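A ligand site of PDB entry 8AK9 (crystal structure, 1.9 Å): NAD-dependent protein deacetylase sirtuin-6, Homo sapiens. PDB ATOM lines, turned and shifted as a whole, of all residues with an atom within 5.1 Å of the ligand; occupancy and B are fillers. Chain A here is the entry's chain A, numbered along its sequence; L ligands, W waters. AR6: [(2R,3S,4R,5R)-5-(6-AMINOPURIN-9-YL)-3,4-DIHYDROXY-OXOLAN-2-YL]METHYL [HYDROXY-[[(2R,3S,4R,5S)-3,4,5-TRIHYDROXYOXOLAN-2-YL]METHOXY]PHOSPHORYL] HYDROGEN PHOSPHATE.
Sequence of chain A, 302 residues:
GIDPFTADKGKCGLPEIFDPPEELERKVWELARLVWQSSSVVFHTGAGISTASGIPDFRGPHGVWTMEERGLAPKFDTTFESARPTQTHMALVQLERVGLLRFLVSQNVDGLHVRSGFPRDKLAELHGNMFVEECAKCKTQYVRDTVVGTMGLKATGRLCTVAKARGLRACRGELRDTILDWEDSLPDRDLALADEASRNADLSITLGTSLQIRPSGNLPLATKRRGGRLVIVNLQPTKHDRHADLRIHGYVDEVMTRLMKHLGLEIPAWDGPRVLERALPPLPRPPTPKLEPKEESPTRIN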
ATOM      1  N   GLU A  16     -19.003  23.955  -9.640  1.00  0.00           N
ATOM      2  CA  GLU A  16     -20.294  23.543  -9.063  1.00  0.00           C
ATOM      3  C   GLU A  16     -20.888  22.431  -9.933  1.00  0.00           C
ATOM      4  O   GLU A  16     -20.574  22.379 -11.125  1.00  0.00           O
ATOM      5  CB  GLU A  16     -21.185  24.763  -8.895  1.00  0.00           C
ATOM      6  CG  GLU A  16     -20.662  25.709  -7.841  1.00  0.00           C
ATOM      7  CD  GLU A  16     -21.550  26.912  -7.676  1.00  0.00           C
ATOM      8  OE1 GLU A  16     -22.087  27.369  -8.696  1.00  0.00           O
ATOM      9  OE2 GLU A  16     -21.724  27.384  -6.526  1.00  0.00           O
ATOM     10  N   GLY A  46     -21.907  23.534   7.398  1.00  0.00           N
ATOM     11  CA  GLY A  46     -20.791  24.415   7.043  1.00  0.00           C
ATOM     12  C   GLY A  46     -21.363  25.587   6.242  1.00  0.00           C
ATOM     13  O   GLY A  46     -22.624  25.654   6.122  1.00  0.00           O
ATOM     14  N   ALA A  47     -20.500  26.445   5.746  1.00  0.00           N
ATOM     15  CA  ALA A  47     -20.760  27.871   5.453  1.00  0.00           C
ATOM     16  C   ALA A  47     -21.745  28.030   4.294  1.00  0.00           C
ATOM     17  O   ALA A  47     -22.337  29.129   4.206  1.00  0.00           O
ATOM     18  CB  ALA A  47     -19.469  28.585   5.166  1.00  0.00           C
ATOM     19  N   GLY A  48     -21.910  26.986   3.485  1.00  0.00           N
ATOM     20  CA  GLY A  48     -22.889  26.861   2.384  1.00  0.00           C
ATOM     21  C   GLY A  48     -24.341  27.007   2.826  1.00  0.00           C
ATOM     22  O   GLY A  48     -25.163  27.512   2.014  1.00  0.00           O
ATOM     23  N   THR A  51     -24.880  31.069   2.828  1.00  0.00           N
ATOM     24  CA  THR A  51     -24.615  31.879   1.608  1.00  0.00           C
ATOM     25  C   THR A  51     -25.892  32.611   1.182  1.00  0.00           C
ATOM     26  O   THR A  51     -25.748  33.749   0.757  1.00  0.00           O
ATOM     27  CB  THR A  51     -24.009  31.079   0.457  1.00  0.00           C
ATOM     28  OG1 THR A  51     -24.740  29.885   0.208  1.00  0.00           O
ATOM     29  CG2 THR A  51     -22.525  30.773   0.634  1.00  0.00           C
ATOM     30  N   ASP A  57     -19.195  31.823   1.691  1.00  0.00           N
ATOM     31  CA  ASP A  57     -18.512  30.603   2.213  1.00  0.00           C
ATOM     32  C   ASP A  57     -16.992  30.791   2.070  1.00  0.00           C
ATOM     33  O   ASP A  57     -16.526  31.945   1.837  1.00  0.00           O
ATOM     34  CB  ASP A  57     -19.075  29.346   1.563  1.00  0.00           C
ATOM     35  CG  ASP A  57     -18.835  29.246   0.065  1.00  0.00           C
ATOM     36  OD1 ASP A  57     -17.930  29.905  -0.401  1.00  0.00           O
ATOM     37  OD2 ASP A  57     -19.560  28.498  -0.608  1.00  0.00           O
ATOM     38  N   PHE A  58     -16.222  29.722   2.270  1.00  0.00           N
ATOM     39  CA  PHE A  58     -14.735  29.767   2.222  1.00  0.00           C
ATOM     40  C   PHE A  58     -14.235  29.322   0.858  1.00  0.00           C
ATOM     41  O   PHE A  58     -13.274  29.927   0.391  1.00  0.00           O
ATOM     42  CB  PHE A  58     -14.132  28.992   3.396  1.00  0.00           C
ATOM     43  CG  PHE A  58     -14.520  29.604   4.722  1.00  0.00           C
ATOM     44  CD1 PHE A  58     -13.805  30.655   5.261  1.00  0.00           C
ATOM     45  CD2 PHE A  58     -15.637  29.153   5.427  1.00  0.00           C
ATOM     46  CE1 PHE A  58     -14.192  31.268   6.443  1.00  0.00           C
ATOM     47  CE2 PHE A  58     -16.020  29.750   6.606  1.00  0.00           C
ATOM     48  CZ  PHE A  58     -15.292  30.807   7.125  1.00  0.00           C
ATOM     49  N   ARG A  59     -14.814  28.284   0.239  1.00  0.00           N
ATOM     50  CA  ARG A  59     -14.140  27.561  -0.861  1.00  0.00           C
ATOM     51  C   ARG A  59     -15.012  27.447  -2.101  1.00  0.00           C
ATOM     52  O   ARG A  59     -14.540  26.822  -3.074  1.00  0.00           O
ATOM     53  CB  ARG A  59     -13.627  26.199  -0.420  1.00  0.00           C
ATOM     54  CG  ARG A  59     -12.784  26.320   0.849  1.00  0.00           C
ATOM     55  CD  ARG A  59     -12.130  25.005   1.224  1.00  0.00           C
ATOM     56  NE  ARG A  59     -11.319  25.186   2.416  1.00  0.00           N
ATOM     57  CZ  ARG A  59     -11.790  25.364   3.662  1.00  0.00           C
ATOM     58  NH1 ARG A  59     -13.090  25.376   3.920  1.00  0.00           N
ATOM     59  NH2 ARG A  59     -10.928  25.480   4.672  1.00  0.00           N
ATOM     60  N   GLY A  60     -16.200  28.043  -2.074  1.00  0.00           N
ATOM     61  CA  GLY A  60     -17.089  28.140  -3.240  1.00  0.00           C
ATOM     62  C   GLY A  60     -16.514  29.127  -4.247  1.00  0.00           C
ATOM     63  O   GLY A  60     -15.481  29.728  -4.008  1.00  0.00           O
ATOM     64  N   TRP A  65     -11.428  32.263   0.920  1.00  0.00           N
ATOM     65  CA  TRP A  65     -10.141  31.694   0.441  1.00  0.00           C
ATOM     66  C   TRP A  65     -10.052  31.691  -1.102  1.00  0.00           C
ATOM     67  O   TRP A  65      -8.972  31.971  -1.622  1.00  0.00           O
ATOM     68  CB  TRP A  65      -9.916  30.279   0.980  1.00  0.00           C
ATOM     69  CG  TRP A  65     -10.030  30.108   2.469  1.00  0.00           C
ATOM     70  CD1 TRP A  65     -10.349  28.940   3.099  1.00  0.00           C
ATOM     71  CD2 TRP A  65      -9.869  31.096   3.497  1.00  0.00           C
ATOM     72  NE1 TRP A  65     -10.395  29.121   4.459  1.00  0.00           N
ATOM     73  CE2 TRP A  65     -10.097  30.430   4.730  1.00  0.00           C
ATOM     74  CE3 TRP A  65      -9.527  32.454   3.527  1.00  0.00           C
ATOM     75  CZ2 TRP A  65      -9.995  31.083   5.963  1.00  0.00           C
ATOM     76  CZ3 TRP A  65      -9.454  33.111   4.738  1.00  0.00           C
ATOM     77  CH2 TRP A  65      -9.684  32.426   5.938  1.00  0.00           C
ATOM     78  N   GLN A 107     -19.662  23.670  11.787  1.00  0.00           N
ATOM     79  CA  GLN A 107     -18.379  24.377  11.643  1.00  0.00           C
ATOM     80  C   GLN A 107     -18.599  25.884  11.588  1.00  0.00           C
ATOM     81  O   GLN A 107     -17.607  26.606  11.625  1.00  0.00           O
ATOM     82  CB  GLN A 107     -17.734  23.811  10.398  1.00  0.00           C
ATOM     83  CG  GLN A 107     -17.283  22.374  10.609  1.00  0.00           C
ATOM     84  CD  GLN A 107     -16.940  21.776   9.284  1.00  0.00           C
ATOM     85  OE1 GLN A 107     -15.833  21.958   8.775  1.00  0.00           O
ATOM     86  NE2 GLN A 107     -17.891  21.039   8.722  1.00  0.00           N
ATOM     87  N   ASN A 108     -19.856  26.358  11.505  1.00  0.00           N
ATOM     88  CA  ASN A 108     -20.106  27.813  11.297  1.00  0.00           C
ATOM     89  C   ASN A 108     -19.931  28.578  12.595  1.00  0.00           C
ATOM     90  O   ASN A 108     -20.470  28.139  13.621  1.00  0.00           O
ATOM     91  CB  ASN A 108     -21.492  28.094  10.715  1.00  0.00           C
ATOM     92  CG  ASN A 108     -21.652  27.357   9.415  1.00  0.00           C
ATOM     93  OD1 ASN A 108     -20.683  27.132   8.736  1.00  0.00           O
ATOM     94  ND2 ASN A 108     -22.848  26.961   9.071  1.00  0.00           N
ATOM     95  N   HIS A 127     -16.162  25.299  15.676  1.00  0.00           N
ATOM     96  CA  HIS A 127     -15.188  26.371  15.393  1.00  0.00           C
ATOM     97  C   HIS A 127     -15.531  27.624  16.180  1.00  0.00           C
ATOM     98  O   HIS A 127     -14.880  28.637  15.920  1.00  0.00           O
ATOM     99  CB  HIS A 127     -15.101  26.644  13.878  1.00  0.00           C
ATOM    100  CG  HIS A 127     -14.702  25.427  13.127  1.00  0.00           C
ATOM    101  ND1 HIS A 127     -14.790  25.325  11.727  1.00  0.00           N
ATOM    102  CD2 HIS A 127     -14.203  24.256  13.588  1.00  0.00           C
ATOM    103  CE1 HIS A 127     -14.365  24.142  11.371  1.00  0.00           C
ATOM    104  NE2 HIS A 127     -14.057  23.429  12.518  1.00  0.00           N
ATOM    105  N   TRP A 182      -6.239  28.936  13.621  1.00  0.00           N
ATOM    106  CA  TRP A 182      -5.731  27.739  12.884  1.00  0.00           C
ATOM    107  C   TRP A 182      -5.120  26.729  13.873  1.00  0.00           C
ATOM    108  O   TRP A 182      -5.439  25.525  13.735  1.00  0.00           O
ATOM    109  CB  TRP A 182      -4.735  28.149  11.787  1.00  0.00           C
ATOM    110  CG  TRP A 182      -5.418  28.726  10.583  1.00  0.00           C
ATOM    111  CD1 TRP A 182      -5.516  30.051  10.241  1.00  0.00           C
ATOM    112  CD2 TRP A 182      -6.172  28.003   9.591  1.00  0.00           C
ATOM    113  NE1 TRP A 182      -6.241  30.198   9.088  1.00  0.00           N
ATOM    114  CE2 TRP A 182      -6.669  28.960   8.668  1.00  0.00           C
ATOM    115  CE3 TRP A 182      -6.453  26.652   9.378  1.00  0.00           C
ATOM    116  CZ2 TRP A 182      -7.425  28.597   7.560  1.00  0.00           C
ATOM    117  CZ3 TRP A 182      -7.209  26.286   8.284  1.00  0.00           C
ATOM    118  CH2 TRP A 182      -7.688  27.250   7.385  1.00  0.00           C
ATOM    119  N   GLY A 208     -23.953  21.901   2.835  1.00  0.00           N
ATOM    120  CA  GLY A 208     -23.128  23.072   2.493  1.00  0.00           C
ATOM    121  C   GLY A 208     -21.804  23.065   3.244  1.00  0.00           C
ATOM    122  O   GLY A 208     -21.352  24.151   3.674  1.00  0.00           O
ATOM    123  N   THR A 209     -21.171  21.891   3.370  1.00  0.00           N
ATOM    124  CA  THR A 209     -19.762  21.769   3.815  1.00  0.00           C
ATOM    125  C   THR A 209     -18.974  20.985   2.758  1.00  0.00           C
ATOM    126  O   THR A 209     -19.504  20.043   2.194  1.00  0.00           O
ATOM    127  CB  THR A 209     -19.643  21.132   5.200  1.00  0.00           C
ATOM    128  OG1 THR A 209     -18.251  21.005   5.478  1.00  0.00           O
ATOM    129  CG2 THR A 209     -20.338  19.792   5.293  1.00  0.00           C
ATOM    130  N   SER A 210     -17.702  21.355   2.540  1.00  0.00           N
ATOM    131  CA  SER A 210     -16.795  20.637   1.627  1.00  0.00           C
ATOM    132  C   SER A 210     -15.991  19.581   2.420  1.00  0.00           C
ATOM    133  O   SER A 210     -15.280  18.840   1.785  1.00  0.00           O
ATOM    134  CB  SER A 210     -15.909  21.605   0.835  1.00  0.00           C
ATOM    135  OG  SER A 210     -15.064  22.385   1.682  1.00  0.00           O
ATOM    136  N   LEU A 211     -16.153  19.477   3.740  1.00  0.00           N
ATOM    137  CA  LEU A 211     -15.645  18.347   4.567  1.00  0.00           C
ATOM    138  C   LEU A 211     -14.123  18.176   4.461  1.00  0.00           C
ATOM    139  O   LEU A 211     -13.636  17.035   4.560  1.00  0.00           O
ATOM    140  CB  LEU A 211     -16.368  17.077   4.111  1.00  0.00           C
ATOM    141  CG  LEU A 211     -17.890  17.116   4.251  1.00  0.00           C
ATOM    142  CD1 LEU A 211     -18.540  15.943   3.527  1.00  0.00           C
ATOM    143  CD2 LEU A 211     -18.280  17.139   5.731  1.00  0.00           C
ATOM    144  N   GLN A 212     -13.391  19.281   4.385  1.00  0.00           N
ATOM    145  CA  GLN A 212     -11.928  19.270   4.112  1.00  0.00           C
ATOM    146  C   GLN A 212     -11.142  19.440   5.409  1.00  0.00           C
ATOM    147  O   GLN A 212      -9.927  19.283   5.367  1.00  0.00           O
ATOM    148  CB  GLN A 212     -11.588  20.369   3.110  1.00  0.00           C
ATOM    149  CG  GLN A 212     -11.988  20.038   1.688  1.00  0.00           C
ATOM    150  CD  GLN A 212     -11.465  21.112   0.775  1.00  0.00           C
ATOM    151  OE1 GLN A 212     -10.264  21.272   0.617  1.00  0.00           O
ATOM    152  NE2 GLN A 212     -12.367  21.852   0.139  1.00  0.00           N
ATOM    153  N   ILE A 213     -11.820  19.759   6.523  1.00  0.00           N
ATOM    154  CA  ILE A 213     -11.149  20.187   7.776  1.00  0.00           C
ATOM    155  C   ILE A 213     -11.334  19.075   8.801  1.00  0.00           C
ATOM    156  O   ILE A 213     -12.495  18.747   9.117  1.00  0.00           O
ATOM    157  CB  ILE A 213     -11.696  21.546   8.253  1.00  0.00           C
ATOM    158  CG1 ILE A 213     -11.477  22.655   7.214  1.00  0.00           C
ATOM    159  CG2 ILE A 213     -11.114  21.926   9.610  1.00  0.00           C
ATOM    160  CD1 ILE A 213     -10.019  23.029   6.994  1.00  0.00           C
ATOM    161  N   VAL A 233     -25.155  16.938   0.902  1.00  0.00           N
ATOM    162  CA  VAL A 233     -25.827  17.977   0.054  1.00  0.00           C
ATOM    163  C   VAL A 233     -24.802  19.089  -0.120  1.00  0.00           C
ATOM    164  O   VAL A 233     -24.395  19.702   0.849  1.00  0.00           O
ATOM    165  CB  VAL A 233     -27.156  18.416   0.680  1.00  0.00           C
ATOM    166  CG1 VAL A 233     -27.864  19.496  -0.133  1.00  0.00           C
ATOM    167  CG2 VAL A 233     -28.092  17.235   0.909  1.00  0.00           C
ATOM    168  N   ASN A 234     -24.390  19.357  -1.353  1.00  0.00           N
ATOM    169  CA  ASN A 234     -23.306  20.306  -1.618  1.00  0.00           C
ATOM    170  C   ASN A 234     -23.245  20.639  -3.102  1.00  0.00           C
ATOM    171  O   ASN A 234     -23.383  19.707  -3.904  1.00  0.00           O
ATOM    172  CB  ASN A 234     -21.962  19.765  -1.142  1.00  0.00           C
ATOM    173  CG  ASN A 234     -21.055  20.887  -0.750  1.00  0.00           C
ATOM    174  OD1 ASN A 234     -21.315  21.607   0.211  1.00  0.00           O
ATOM    175  ND2 ASN A 234     -19.971  21.067  -1.482  1.00  0.00           N
ATOM    176  N   LEU A 235     -22.946  21.892  -3.445  1.00  0.00           N
ATOM    177  CA  LEU A 235     -22.915  22.310  -4.871  1.00  0.00           C
ATOM    178  C   LEU A 235     -21.602  21.836  -5.519  1.00  0.00           C
ATOM    179  O   LEU A 235     -21.605  21.514  -6.719  1.00  0.00           O
ATOM    180  CB  LEU A 235     -23.082  23.823  -4.931  1.00  0.00           C
ATOM    181  CG  LEU A 235     -24.511  24.317  -4.922  1.00  0.00           C
ATOM    182  CD1 LEU A 235     -24.557  25.826  -4.777  1.00  0.00           C
ATOM    183  CD2 LEU A 235     -25.248  23.871  -6.188  1.00  0.00           C
ATOM    184  N   GLN A 236     -20.547  21.741  -4.721  1.00  0.00           N
ATOM    185  CA  GLN A 236     -19.198  21.323  -5.135  1.00  0.00           C
ATOM    186  C   GLN A 236     -18.938  19.908  -4.625  1.00  0.00           C
ATOM    187  O   GLN A 236     -19.579  19.445  -3.685  1.00  0.00           O
ATOM    188  CB  GLN A 236     -18.126  22.217  -4.534  1.00  0.00           C
ATOM    189  CG  GLN A 236     -18.022  23.601  -5.154  1.00  0.00           C
ATOM    190  CD  GLN A 236     -16.967  24.420  -4.452  1.00  0.00           C
ATOM    191  OE1 GLN A 236     -16.705  24.259  -3.265  1.00  0.00           O
ATOM    192  NE2 GLN A 236     -16.399  25.368  -5.171  1.00  0.00           N
ATOM    193  N   PRO A 237     -17.966  19.206  -5.237  1.00  0.00           N
ATOM    194  CA  PRO A 237     -17.353  18.024  -4.639  1.00  0.00           C
ATOM    195  C   PRO A 237     -16.932  18.257  -3.183  1.00  0.00           C
ATOM    196  O   PRO A 237     -16.652  19.356  -2.828  1.00  0.00           O
ATOM    197  CB  PRO A 237     -16.084  17.812  -5.478  1.00  0.00           C
ATOM    198  CG  PRO A 237     -16.417  18.423  -6.831  1.00  0.00           C
ATOM    199  CD  PRO A 237     -17.438  19.511  -6.575  1.00  0.00           C
ATOM    200  N   GLY A 250     -27.266  20.649  -5.356  1.00  0.00           N
ATOM    201  CA  GLY A 250     -28.352  21.637  -5.400  1.00  0.00           C
ATOM    202  C   GLY A 250     -28.199  22.646  -4.297  1.00  0.00           C
ATOM    203  O   GLY A 250     -27.360  22.429  -3.397  1.00  0.00           O
ATOM    204  N   TYR A 251     -28.909  23.778  -4.404  1.00  0.00           N
ATOM    205  CA  TYR A 251     -29.066  24.784  -3.346  1.00  0.00           C
ATOM    206  C   TYR A 251     -29.730  24.124  -2.162  1.00  0.00           C
ATOM    207  O   TYR A 251     -30.762  23.446  -2.364  1.00  0.00           O
ATOM    208  CB  TYR A 251     -29.902  25.950  -3.847  1.00  0.00           C
ATOM    209  CG  TYR A 251     -29.186  26.655  -4.950  1.00  0.00           C
ATOM    210  CD1 TYR A 251     -28.086  27.446  -4.661  1.00  0.00           C
ATOM    211  CD2 TYR A 251     -29.527  26.457  -6.274  1.00  0.00           C
ATOM    212  CE1 TYR A 251     -27.379  28.083  -5.661  1.00  0.00           C
ATOM    213  CE2 TYR A 251     -28.837  27.099  -7.289  1.00  0.00           C
ATOM    214  CZ  TYR A 251     -27.767  27.928  -6.972  1.00  0.00           C
ATOM    215  OH  TYR A 251     -27.062  28.549  -7.954  1.00  0.00           O
ATOM    216  N   VAL A 252     -29.146  24.302  -0.984  1.00  0.00           N
ATOM    217  CA  VAL A 252     -29.548  23.517   0.208  1.00  0.00           C
ATOM    218  C   VAL A 252     -30.968  23.968   0.582  1.00  0.00           C
ATOM    219  O   VAL A 252     -31.778  23.152   0.966  1.00  0.00           O
ATOM    220  CB  VAL A 252     -28.489  23.630   1.330  1.00  0.00           C
ATOM    221  CG1 VAL A 252     -28.350  25.063   1.863  1.00  0.00           C
ATOM    222  CG2 VAL A 252     -28.788  22.662   2.457  1.00  0.00           C
HETATM  223  N1  AR6 L   1     -26.368  25.140  -1.354  1.00  0.00           N
HETATM  224  C2  AR6 L   1     -25.517  24.103  -1.348  1.00  0.00           C
HETATM  225  N3  AR6 L   1     -24.200  24.098  -1.244  1.00  0.00           N
HETATM  226  C4  AR6 L   1     -23.741  25.345  -1.080  1.00  0.00           C
HETATM  227  C5  AR6 L   1     -24.482  26.512  -1.082  1.00  0.00           C
HETATM  228  C6  AR6 L   1     -25.881  26.382  -1.233  1.00  0.00           C
HETATM  229  N6  AR6 L   1     -26.753  27.400  -1.194  1.00  0.00           N
HETATM  230  N7  AR6 L   1     -23.631  27.598  -0.934  1.00  0.00           N
HETATM  231  C8  AR6 L   1     -22.445  27.077  -0.840  1.00  0.00           C
HETATM  232  N9  AR6 L   1     -22.441  25.726  -0.944  1.00  0.00           N
HETATM  233  PA  AR6 L   1     -16.493  25.539   2.473  1.00  0.00           P
HETATM  234  PB  AR6 L   1     -16.915  24.713   5.302  1.00  0.00           P
HETATM  235  C1' AR6 L   1     -21.296  24.830  -0.810  1.00  0.00           C
HETATM  236  O1A AR6 L   1     -15.249  24.721   2.379  1.00  0.00           O
HETATM  237  O1B AR6 L   1     -18.080  25.089   6.153  1.00  0.00           O
HETATM  238  C1D AR6 L   1     -12.838  27.344   7.159  1.00  0.00           C
HETATM  239  O1D AR6 L   1     -11.483  27.659   7.155  1.00  0.00           O
HETATM  240  C2' AR6 L   1     -20.001  25.186  -1.541  1.00  0.00           C
HETATM  241  O2' AR6 L   1     -20.022  24.607  -2.830  1.00  0.00           O
HETATM  242  O2A AR6 L   1     -16.642  26.868   1.792  1.00  0.00           O
HETATM  243  O2B AR6 L   1     -16.738  23.336   4.797  1.00  0.00           O
HETATM  244  C2D AR6 L   1     -13.558  27.630   8.481  1.00  0.00           C
HETATM  245  O2D AR6 L   1     -12.830  27.296   9.644  1.00  0.00           O
HETATM  246  C3' AR6 L   1     -18.914  24.575  -0.625  1.00  0.00           C
HETATM  247  O3' AR6 L   1     -18.441  23.345  -1.174  1.00  0.00           O
HETATM  248  O3A AR6 L   1     -16.900  25.692   4.011  1.00  0.00           O
HETATM  249  C3D AR6 L   1     -14.766  26.699   8.351  1.00  0.00           C
HETATM  250  O3D AR6 L   1     -15.403  26.447   9.601  1.00  0.00           O
HETATM  251  C4' AR6 L   1     -19.625  24.334   0.712  1.00  0.00           C
HETATM  252  O4' AR6 L   1     -20.922  24.934   0.542  1.00  0.00           O
HETATM  253  C4D AR6 L   1     -14.088  25.440   7.802  1.00  0.00           C
HETATM  254  O4D AR6 L   1     -13.044  25.910   6.933  1.00  0.00           O
HETATM  255  C5' AR6 L   1     -19.022  24.944   1.938  1.00  0.00           C
HETATM  256  O5' AR6 L   1     -17.648  24.558   1.997  1.00  0.00           O
HETATM  257  C5D AR6 L   1     -14.964  24.479   7.030  1.00  0.00           C
HETATM  258  O5D AR6 L   1     -15.566  25.220   5.951  1.00  0.00           O
HETATM  259  O   HOH W   1     -17.880  26.984   8.357  1.00  0.00           O
HETATM  260  O   HOH W   2     -27.495  29.163   1.468  1.00  0.00           O
HETATM  261  O   HOH W   3     -29.612  27.540  -0.379  1.00  0.00           O
HETATM  262  O   HOH W   4     -20.680  26.591  -4.394  1.00  0.00           O
HETATM  263  O   HOH W   5     -20.639  29.066  -3.040  1.00  0.00           O
HETATM  264  O   HOH W   6     -14.246  21.964   4.334  1.00  0.00           O
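Water W4 bridges OE2 of Glu 16 (2.5 Å) and O2' of the ligand (2.6 Å). Water W1 lies within hydrogen-bond range of O3D of the ligand, OD1 of Asn 108 and O of Gln 107. Water W6 lies within hydrogen-bond range of the side-chain hydroxyl of Ser 210 (2.8 Å), the backbone NH of Gln 212 (2.8 Å), an oxygen (O2B) of the ligand (2.9 Å) and the backbone NH of Leu 211 (3.2 Å). Water W3 lies within hydrogen-bond range of N6 of the ligand (3.0 Å) and N of Val 252 (3.3 Å). Water W2 lies within hydrogen-bond range of the backbone carbonyl oxygen of Gly 48 (2.9 Å), the side-chain hydroxyl of Thr 51 (3.1 Å) and a nitrogen (N6) of the ligand (3.3 Å).
The backbone carbonyl oxygen of Gly 48 sits close to a nitrogen (N7) of the ligand (3.3 Å). O4' of the ligand lies close to O of Gly 208 (3.3 Å). Gly 46 touches the ligand (CA to O1B, 2.9 Å). Asp 57 touches the ligand (OD2 to C8, 3.2 Å). Trp 182 touches the ligand. CG1 of Ile 213 touches O4D of the ligand, 3.6 Å away. Gly 250 touches the ligand (O to C2, 3.2 Å). CA of Tyr 251 touches N1 of the ligand, 3.4 Å away. Hydrophobic or aromatic side chains that line the ligand: Ala 47, Phe 58, Trp 65, His 127, Trp 182, Ile 213, Leu 235, Tyr 251 and Val 252. Of the 28 residues printed, 21 come within 4 Å of the ligand.
The indole nitrogen (NE1) of Trp 65 is in hydrogen-bond range of an oxygen (O1D) of the ligand (3.3 Å). N of Ala 47 sits at hydrogen-bond distance from O1B of the ligand (2.8 Å). The backbone NH (N) of Phe 58 lies within hydrogen-bond range of an oxygen (O2A) of the ligand, at 2.9 Å. The guanidinium group of Arg 59 lies within salt-bridge range of an oxygen (O1A) of the ligand, 2.7 Å away. The backbone NH (N) of Val 252 is in hydrogen-bond range of a nitrogen (N1) of the ligand. The side-chain hydroxyl (OG1) of Thr 51 lies within hydrogen-bond range of a nitrogen (N7) of the ligand (2.8 Å). The backbone NH (N) of Leu 235 lies within hydrogen-bond range of a nitrogen (N3) of the ligand, at 3.4 Å. A ring nitrogen (ND1) of His 127 is in hydrogen-bond range of an oxygen (O3D) of the ligand (2.5 Å). The backbone carbonyl oxygen (O) of Gln 107 lies within hydrogen-bond range of an oxygen (O3D) of the ligand. An oxygen (O2B) of the ligand is in hydrogen-bond range of the backbone NH of Ser 210 (3.2 Å). ND2 of Asn 234 sits at hydrogen-bond distance from O3' of the ligand (2.8 Å). OG of Ser 210 lies within hydrogen-bond range of O1A of the ligand (2.4 Å). An oxygen (O2A) of the ligand sits at hydrogen-bond distance from the backbone NH (N) of Arg 59, 2.8 Å away. An oxygen (O3') of the ligand is in hydrogen-bond range of the side-chain amide oxygen of Gln 236 (2.9 Å). N of Gln 236 lies close to O2' of the ligand, 3.5 Å away. The side-chain hydroxyl (OG1) of Thr 209 is in hydrogen-bond range of an oxygen (O2B) of the ligand (2.9 Å).
The backbone carbonyl oxygen (O) of Gln 107 sits at hydrogen-bond distance from a ring nitrogen (ND1) of His 127 (3.1 Å). N of Gly 208 lies within hydrogen-bond range of O of Val 233. O of Phe 58 lies within hydrogen-bond range of N of Trp 65, 3.0 Å away. The backbone NH (N) of Ala 47 lies within hydrogen-bond range of the side-chain amide oxygen (OD1) of Asn 108, at 3.1 Å. The backbone NH of Gly 48 lies within hydrogen-bond range of the backbone carbonyl oxygen of Gly 208 (2.9 Å). O of Gly 48 sits at hydrogen-bond distance from OG1 of Thr 51. The side-chain hydroxyl (OG) of Ser 210 sits at hydrogen-bond distance from the side-chain amide nitrogen (NE2) of Gln 212. The backbone carbonyl oxygen of Gly 208 is in hydrogen-bond range of the backbone NH of Ala 47 (3.2 Å).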
